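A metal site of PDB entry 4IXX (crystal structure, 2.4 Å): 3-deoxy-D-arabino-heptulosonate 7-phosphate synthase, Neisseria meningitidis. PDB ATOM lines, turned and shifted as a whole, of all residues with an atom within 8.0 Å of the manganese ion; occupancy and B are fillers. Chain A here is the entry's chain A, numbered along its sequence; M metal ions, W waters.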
ATOM      1  N   GLY A  61     -12.522   5.396  -1.689  1.00  0.00           N
ATOM      2  CA  GLY A  61     -11.794   4.742  -2.720  1.00  0.00           C
ATOM      3  C   GLY A  61     -11.897   3.233  -2.518  1.00  0.00           C
ATOM      4  O   GLY A  61     -12.731   2.761  -1.784  1.00  0.00           O
ATOM      5  N   PRO A  62     -11.031   2.470  -3.184  1.00  0.00           N
ATOM      6  CA  PRO A  62     -11.126   1.028  -3.140  1.00  0.00           C
ATOM      7  C   PRO A  62     -10.988   0.406  -1.787  1.00  0.00           C
ATOM      8  O   PRO A  62     -10.363   0.936  -0.882  1.00  0.00           O
ATOM      9  CB  PRO A  62      -9.960   0.605  -3.992  1.00  0.00           C
ATOM     10  CG  PRO A  62      -9.819   1.745  -4.983  1.00  0.00           C
ATOM     11  CD  PRO A  62     -10.052   2.958  -4.169  1.00  0.00           C
ATOM     12  N   CYS A  63     -11.659  -0.729  -1.629  1.00  0.00           N
ATOM     13  CA  CYS A  63     -11.513  -1.545  -0.423  1.00  0.00           C
ATOM     14  C   CYS A  63     -10.012  -1.896  -0.271  1.00  0.00           C
ATOM     15  O   CYS A  63      -9.486  -1.839   0.821  1.00  0.00           O
ATOM     16  CB  CYS A  63     -12.331  -2.809  -0.546  1.00  0.00           C
ATOM     17  SG  CYS A  63     -12.000  -3.980   0.804  1.00  0.00           S
ATOM     18  N   SER A  64      -9.375  -2.257  -1.380  1.00  0.00           N
ATOM     19  CA  SER A  64      -7.954  -2.567  -1.357  1.00  0.00           C
ATOM     20  C   SER A  64      -7.351  -2.207  -2.680  1.00  0.00           C
ATOM     21  O   SER A  64      -8.020  -2.307  -3.712  1.00  0.00           O
ATOM     22  CB  SER A  64      -7.717  -4.042  -1.082  1.00  0.00           C
ATOM     23  OG  SER A  64      -8.293  -4.809  -2.110  1.00  0.00           O
ATOM     24  N   ARG A  94      -8.763   6.411  -0.279  1.00  0.00           N
ATOM     25  CA  ARG A  94      -8.483   5.149   0.391  1.00  0.00           C
ATOM     26  C   ARG A  94      -7.409   4.470  -0.388  1.00  0.00           C
ATOM     27  O   ARG A  94      -7.628   4.117  -1.526  1.00  0.00           O
ATOM     28  CB  ARG A  94      -9.672   4.196   0.356  1.00  0.00           C
ATOM     29  CG  ARG A  94     -10.682   4.374   1.438  1.00  0.00           C
ATOM     30  CD  ARG A  94     -11.793   3.321   1.286  1.00  0.00           C
ATOM     31  NE  ARG A  94     -11.326   1.945   1.515  1.00  0.00           N
ATOM     32  CZ  ARG A  94     -11.448   1.287   2.660  1.00  0.00           C
ATOM     33  NH1 ARG A  94     -12.045   1.850   3.703  1.00  0.00           N
ATOM     34  NH2 ARG A  94     -10.936   0.051   2.788  1.00  0.00           N
ATOM     35  N   TYR A  96      -5.544   1.442   0.591  1.00  0.00           N
ATOM     36  CA  TYR A  96      -5.322   0.366   1.579  1.00  0.00           C
ATOM     37  C   TYR A  96      -4.449  -0.756   1.005  1.00  0.00           C
ATOM     38  O   TYR A  96      -4.844  -1.456   0.084  1.00  0.00           O
ATOM     39  CB  TYR A  96      -6.667  -0.190   2.086  1.00  0.00           C
ATOM     40  CG  TYR A  96      -7.395   0.665   3.128  1.00  0.00           C
ATOM     41  CD1 TYR A  96      -7.517   2.039   2.989  1.00  0.00           C
ATOM     42  CD2 TYR A  96      -8.004   0.081   4.220  1.00  0.00           C
ATOM     43  CE1 TYR A  96      -8.202   2.800   3.950  1.00  0.00           C
ATOM     44  CE2 TYR A  96      -8.701   0.816   5.162  1.00  0.00           C
ATOM     45  CZ  TYR A  96      -8.772   2.182   5.038  1.00  0.00           C
ATOM     46  OH  TYR A  96      -9.458   2.888   6.000  1.00  0.00           O
ATOM     47  N   LYS A  99      -4.954  -5.951   4.404  1.00  0.00           N
ATOM     48  CA  LYS A  99      -6.335  -6.408   4.640  1.00  0.00           C
ATOM     49  C   LYS A  99      -6.414  -7.523   5.636  1.00  0.00           C
ATOM     50  O   LYS A  99      -5.854  -8.590   5.427  1.00  0.00           O
ATOM     51  CB  LYS A  99      -6.963  -6.916   3.349  1.00  0.00           C
ATOM     52  CG  LYS A  99      -6.912  -5.913   2.218  1.00  0.00           C
ATOM     53  CD  LYS A  99      -7.497  -4.549   2.602  1.00  0.00           C
ATOM     54  CE  LYS A  99      -8.999  -4.625   2.923  1.00  0.00           C
ATOM     55  NZ  LYS A  99      -9.603  -3.284   3.119  1.00  0.00           N
ATOM     56  N   PRO A 100      -7.166  -7.301   6.725  1.00  0.00           N
ATOM     57  CA  PRO A 100      -7.393  -8.374   7.695  1.00  0.00           C
ATOM     58  C   PRO A 100      -8.474  -9.294   7.194  1.00  0.00           C
ATOM     59  O   PRO A 100      -9.562  -8.867   6.900  1.00  0.00           O
ATOM     60  CB  PRO A 100      -7.888  -7.628   8.924  1.00  0.00           C
ATOM     61  CG  PRO A 100      -8.429  -6.326   8.428  1.00  0.00           C
ATOM     62  CD  PRO A 100      -7.909  -6.081   7.048  1.00  0.00           C
ATOM     63  N   GLU A 145      -5.171   1.614   6.285  1.00  0.00           N
ATOM     64  CA  GLU A 145      -5.324   0.870   7.530  1.00  0.00           C
ATOM     65  C   GLU A 145      -3.942   0.395   7.945  1.00  0.00           C
ATOM     66  O   GLU A 145      -3.198  -0.194   7.149  1.00  0.00           O
ATOM     67  CB  GLU A 145      -6.311  -0.325   7.445  1.00  0.00           C
ATOM     68  CG  GLU A 145      -6.288  -1.161   8.717  1.00  0.00           C
ATOM     69  CD  GLU A 145      -7.260  -2.362   8.831  1.00  0.00           C
ATOM     70  OE1 GLU A 145      -8.267  -2.455   8.083  1.00  0.00           O
ATOM     71  OE2 GLU A 145      -7.030  -3.198   9.767  1.00  0.00           O
ATOM     72  N   ARG A 167     -11.039  -5.283  13.878  1.00  0.00           N
ATOM     73  CA  ARG A 167     -10.468  -6.503  14.466  1.00  0.00           C
ATOM     74  C   ARG A 167      -9.271  -6.274  15.345  1.00  0.00           C
ATOM     75  O   ARG A 167      -8.800  -7.208  15.992  1.00  0.00           O
ATOM     76  CB  ARG A 167     -10.120  -7.507  13.345  1.00  0.00           C
ATOM     77  CG  ARG A 167     -11.365  -8.089  12.650  1.00  0.00           C
ATOM     78  CD  ARG A 167     -11.083  -8.859  11.353  1.00  0.00           C
ATOM     79  NE  ARG A 167     -12.336  -9.176  10.617  1.00  0.00           N
ATOM     80  CZ  ARG A 167     -13.068  -8.312   9.868  1.00  0.00           C
ATOM     81  NH1 ARG A 167     -12.725  -7.020   9.739  1.00  0.00           N
ATOM     82  NH2 ARG A 167     -14.156  -8.738   9.240  1.00  0.00           N
ATOM     83  N   LYS A 188     -12.111   1.852  14.514  1.00  0.00           N
ATOM     84  CA  LYS A 188     -13.450   1.249  14.299  1.00  0.00           C
ATOM     85  C   LYS A 188     -14.041   0.527  15.478  1.00  0.00           C
ATOM     86  O   LYS A 188     -13.339  -0.033  16.298  1.00  0.00           O
ATOM     87  CB  LYS A 188     -13.401   0.311  13.150  1.00  0.00           C
ATOM     88  CG  LYS A 188     -13.137   1.073  11.883  1.00  0.00           C
ATOM     89  CD  LYS A 188     -13.206   0.218  10.667  1.00  0.00           C
ATOM     90  CE  LYS A 188     -13.672   1.063   9.528  1.00  0.00           C
ATOM     91  NZ  LYS A 188     -14.117   0.275   8.365  1.00  0.00           N
ATOM     92  N   ASP A 267     -18.846   4.868   8.658  1.00  0.00           N
ATOM     93  CA  ASP A 267     -18.500   4.082   7.500  1.00  0.00           C
ATOM     94  C   ASP A 267     -19.813   3.735   6.810  1.00  0.00           C
ATOM     95  O   ASP A 267     -20.685   3.117   7.419  1.00  0.00           O
ATOM     96  CB  ASP A 267     -17.697   2.829   7.930  1.00  0.00           C
ATOM     97  CG  ASP A 267     -17.171   2.018   6.781  1.00  0.00           C
ATOM     98  OD1 ASP A 267     -17.413   2.351   5.608  1.00  0.00           O
ATOM     99  OD2 ASP A 267     -16.569   0.934   7.053  1.00  0.00           O
ATOM    100  N   SER A 269     -19.978   1.609   4.389  1.00  0.00           N
ATOM    101  CA  SER A 269     -19.836   0.221   3.880  1.00  0.00           C
ATOM    102  C   SER A 269     -19.756  -0.802   5.015  1.00  0.00           C
ATOM    103  O   SER A 269     -20.277  -0.603   6.099  1.00  0.00           O
ATOM    104  CB  SER A 269     -18.585   0.132   3.026  1.00  0.00           C
ATOM    105  OG  SER A 269     -18.596  -0.995   2.187  1.00  0.00           O
ATOM    106  N   HIS A 270     -19.086  -1.920   4.746  1.00  0.00           N
ATOM    107  CA  HIS A 270     -18.944  -2.997   5.697  1.00  0.00           C
ATOM    108  C   HIS A 270     -20.267  -3.356   6.392  1.00  0.00           C
ATOM    109  O   HIS A 270     -21.272  -3.590   5.699  1.00  0.00           O
ATOM    110  CB  HIS A 270     -17.819  -2.670   6.639  1.00  0.00           C
ATOM    111  CG  HIS A 270     -16.532  -2.449   5.917  1.00  0.00           C
ATOM    112  ND1 HIS A 270     -16.050  -1.187   5.617  1.00  0.00           N
ATOM    113  CD2 HIS A 270     -15.723  -3.319   5.280  1.00  0.00           C
ATOM    114  CE1 HIS A 270     -14.992  -1.308   4.841  1.00  0.00           C
ATOM    115  NE2 HIS A 270     -14.780  -2.586   4.623  1.00  0.00           N
ATOM    116  N   LYS A 275     -22.566  -5.277   3.610  1.00  0.00           N
ATOM    117  CA  LYS A 275     -21.685  -5.780   2.536  1.00  0.00           C
ATOM    118  C   LYS A 275     -22.358  -5.761   1.164  1.00  0.00           C
ATOM    119  O   LYS A 275     -22.018  -6.529   0.280  1.00  0.00           O
ATOM    120  CB  LYS A 275     -21.147  -7.168   2.916  1.00  0.00           C
ATOM    121  CG  LYS A 275     -20.461  -7.183   4.279  1.00  0.00           C
ATOM    122  CD  LYS A 275     -19.433  -8.323   4.401  1.00  0.00           C
ATOM    123  CE  LYS A 275     -20.116  -9.659   4.626  1.00  0.00           C
ATOM    124  NZ  LYS A 275     -19.129 -10.693   5.058  1.00  0.00           N
ATOM    125  N   MET A 302     -16.918   7.341   5.371  1.00  0.00           N
ATOM    126  CA  MET A 302     -16.021   6.424   4.678  1.00  0.00           C
ATOM    127  C   MET A 302     -16.867   5.700   3.612  1.00  0.00           C
ATOM    128  O   MET A 302     -17.999   5.322   3.859  1.00  0.00           O
ATOM    129  CB  MET A 302     -15.378   5.483   5.715  1.00  0.00           C
ATOM    130  CG  MET A 302     -14.580   4.329   5.146  1.00  0.00           C
ATOM    131  SD  MET A 302     -13.731   3.351   6.431  1.00  0.00           S
ATOM    132  CE  MET A 302     -12.516   4.518   7.033  1.00  0.00           C
ATOM    133  N   GLU A 304     -16.644   2.764   0.127  1.00  0.00           N
ATOM    134  CA  GLU A 304     -15.619   1.955  -0.621  1.00  0.00           C
ATOM    135  C   GLU A 304     -16.151   2.044  -2.043  1.00  0.00           C
ATOM    136  O   GLU A 304     -17.309   1.687  -2.427  1.00  0.00           O
ATOM    137  CB  GLU A 304     -15.862   0.425  -0.032  1.00  0.00           C
ATOM    138  CG  GLU A 304     -15.124   0.338   1.194  1.00  0.00           C
ATOM    139  CD  GLU A 304     -14.966  -1.084   1.611  1.00  0.00           C
ATOM    140  OE1 GLU A 304     -15.964  -1.779   1.667  1.00  0.00           O
ATOM    141  OE2 GLU A 304     -13.891  -1.566   1.950  1.00  0.00           O
ATOM    142  N   SER A 321     -12.834  -4.269  -7.653  1.00  0.00           N
ATOM    143  CA  SER A 321     -12.311  -4.801  -6.403  1.00  0.00           C
ATOM    144  C   SER A 321     -12.223  -6.301  -6.383  1.00  0.00           C
ATOM    145  O   SER A 321     -13.110  -6.976  -6.904  1.00  0.00           O
ATOM    146  CB  SER A 321     -13.166  -4.301  -5.215  1.00  0.00           C
ATOM    147  OG  SER A 321     -12.766  -4.960  -4.003  1.00  0.00           O
ATOM    148  N   THR A 323     -11.538  -7.613  -3.189  1.00  0.00           N
ATOM    149  CA  THR A 323     -11.930  -7.785  -1.792  1.00  0.00           C
ATOM    150  C   THR A 323     -13.405  -7.305  -1.632  1.00  0.00           C
ATOM    151  O   THR A 323     -14.241  -7.800  -2.358  1.00  0.00           O
ATOM    152  CB  THR A 323     -10.908  -7.093  -0.858  1.00  0.00           C
ATOM    153  OG1 THR A 323     -10.575  -5.763  -1.314  1.00  0.00           O
ATOM    154  CG2 THR A 323      -9.646  -7.926  -0.853  1.00  0.00           C
ATOM    155  N   ASP A 324     -13.759  -6.408  -0.774  1.00  0.00           N
ATOM    156  CA  ASP A 324     -15.153  -5.967  -0.634  1.00  0.00           C
ATOM    157  C   ASP A 324     -15.698  -5.267  -1.831  1.00  0.00           C
ATOM    158  O   ASP A 324     -14.977  -4.507  -2.472  1.00  0.00           O
ATOM    159  CB  ASP A 324     -15.491  -5.049   0.518  1.00  0.00           C
ATOM    160  CG  ASP A 324     -15.183  -5.670   1.869  1.00  0.00           C
ATOM    161  OD1 ASP A 324     -15.346  -6.902   2.006  1.00  0.00           O
ATOM    162  OD2 ASP A 324     -14.771  -4.931   2.791  1.00  0.00           O
ATOM    163  N   ALA A 325     -16.975  -5.492  -2.169  1.00  0.00           N
ATOM    164  CA  ALA A 325     -17.550  -4.900  -3.328  1.00  0.00           C
ATOM    165  C   ALA A 325     -17.611  -3.388  -3.154  1.00  0.00           C
ATOM    166  O   ALA A 325     -17.932  -2.923  -2.041  1.00  0.00           O
ATOM    167  CB  ALA A 325     -18.947  -5.454  -3.628  1.00  0.00           C
ATOM    168  N   CYS A 326     -17.323  -2.659  -4.243  1.00  0.00           N
ATOM    169  CA  CYS A 326     -17.403  -1.229  -4.236  1.00  0.00           C
ATOM    170  C   CYS A 326     -18.515  -0.644  -5.123  1.00  0.00           C
ATOM    171  O   CYS A 326     -19.013  -1.308  -6.043  1.00  0.00           O
ATOM    172  CB  CYS A 326     -16.041  -0.664  -4.645  1.00  0.00           C
ATOM    173  SG  CYS A 326     -14.718  -1.280  -3.541  1.00  0.00           S
HETATM  174 MN    MN M   1     -13.324  -3.385   3.045  1.00  0.00          MN
HETATM  175  O   HOH W   1     -11.810  -1.542   4.972  1.00  0.00           O
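The backbone carbonyl oxygen (O) of Asp 324 is in hydrogen-bond range of the side-chain sulfur (SG) of Cys 326, at 3.4 Å.
The side-chain carboxylate of Glu 304 lies close to the guanidinium group of Arg 94 (3.5 Å).
The side-chain carboxylate (OE1) of Glu 304 lies within hydrogen-bond range of the side-chain hydroxyl (OG) of Ser 269, at 2.8 Å.
The side-chain carboxylate (OD2) of Asp 267 is in hydrogen-bond range of a ring nitrogen (ND1) of His 270.
The backbone carbonyl oxygen (O) of Cys 63 lies within hydrogen-bond range of the side-chain amino group (NZ) of Lys 99, 2.7 Å away.
The backbone carbonyl oxygen of Cys 63 sits at hydrogen-bond distance from the guanidinium group of Arg 94 (3.1 Å).
The side-chain sulfur of Cys 63 lies close to the side-chain hydroxyl of Thr 323, 3.1 Å away.
The side-chain sulfur (SG) of Cys 326 sits at hydrogen-bond distance from the backbone NH (N) of Cys 63, 3.6 Å away.
Lys 99 touches the manganese ion (NZ to MN, 3.7 Å).
Within 4 Å of the manganese ion: Cys 63, Lys 99, His 270, Glu 304 and Asp 324.
The manganese ion is bound by the side-chain carboxylate of Asp 324 (2.1 Å), the side-chain carboxylate of Glu 304 (2.2 Å), a ring nitrogen (NE2) of His 270 (2.3 Å) and the side-chain sulfur of Cys 63 (2.7 Å).
Water W1 bridges NH2 of Arg 94 and NZ of Lys 99.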
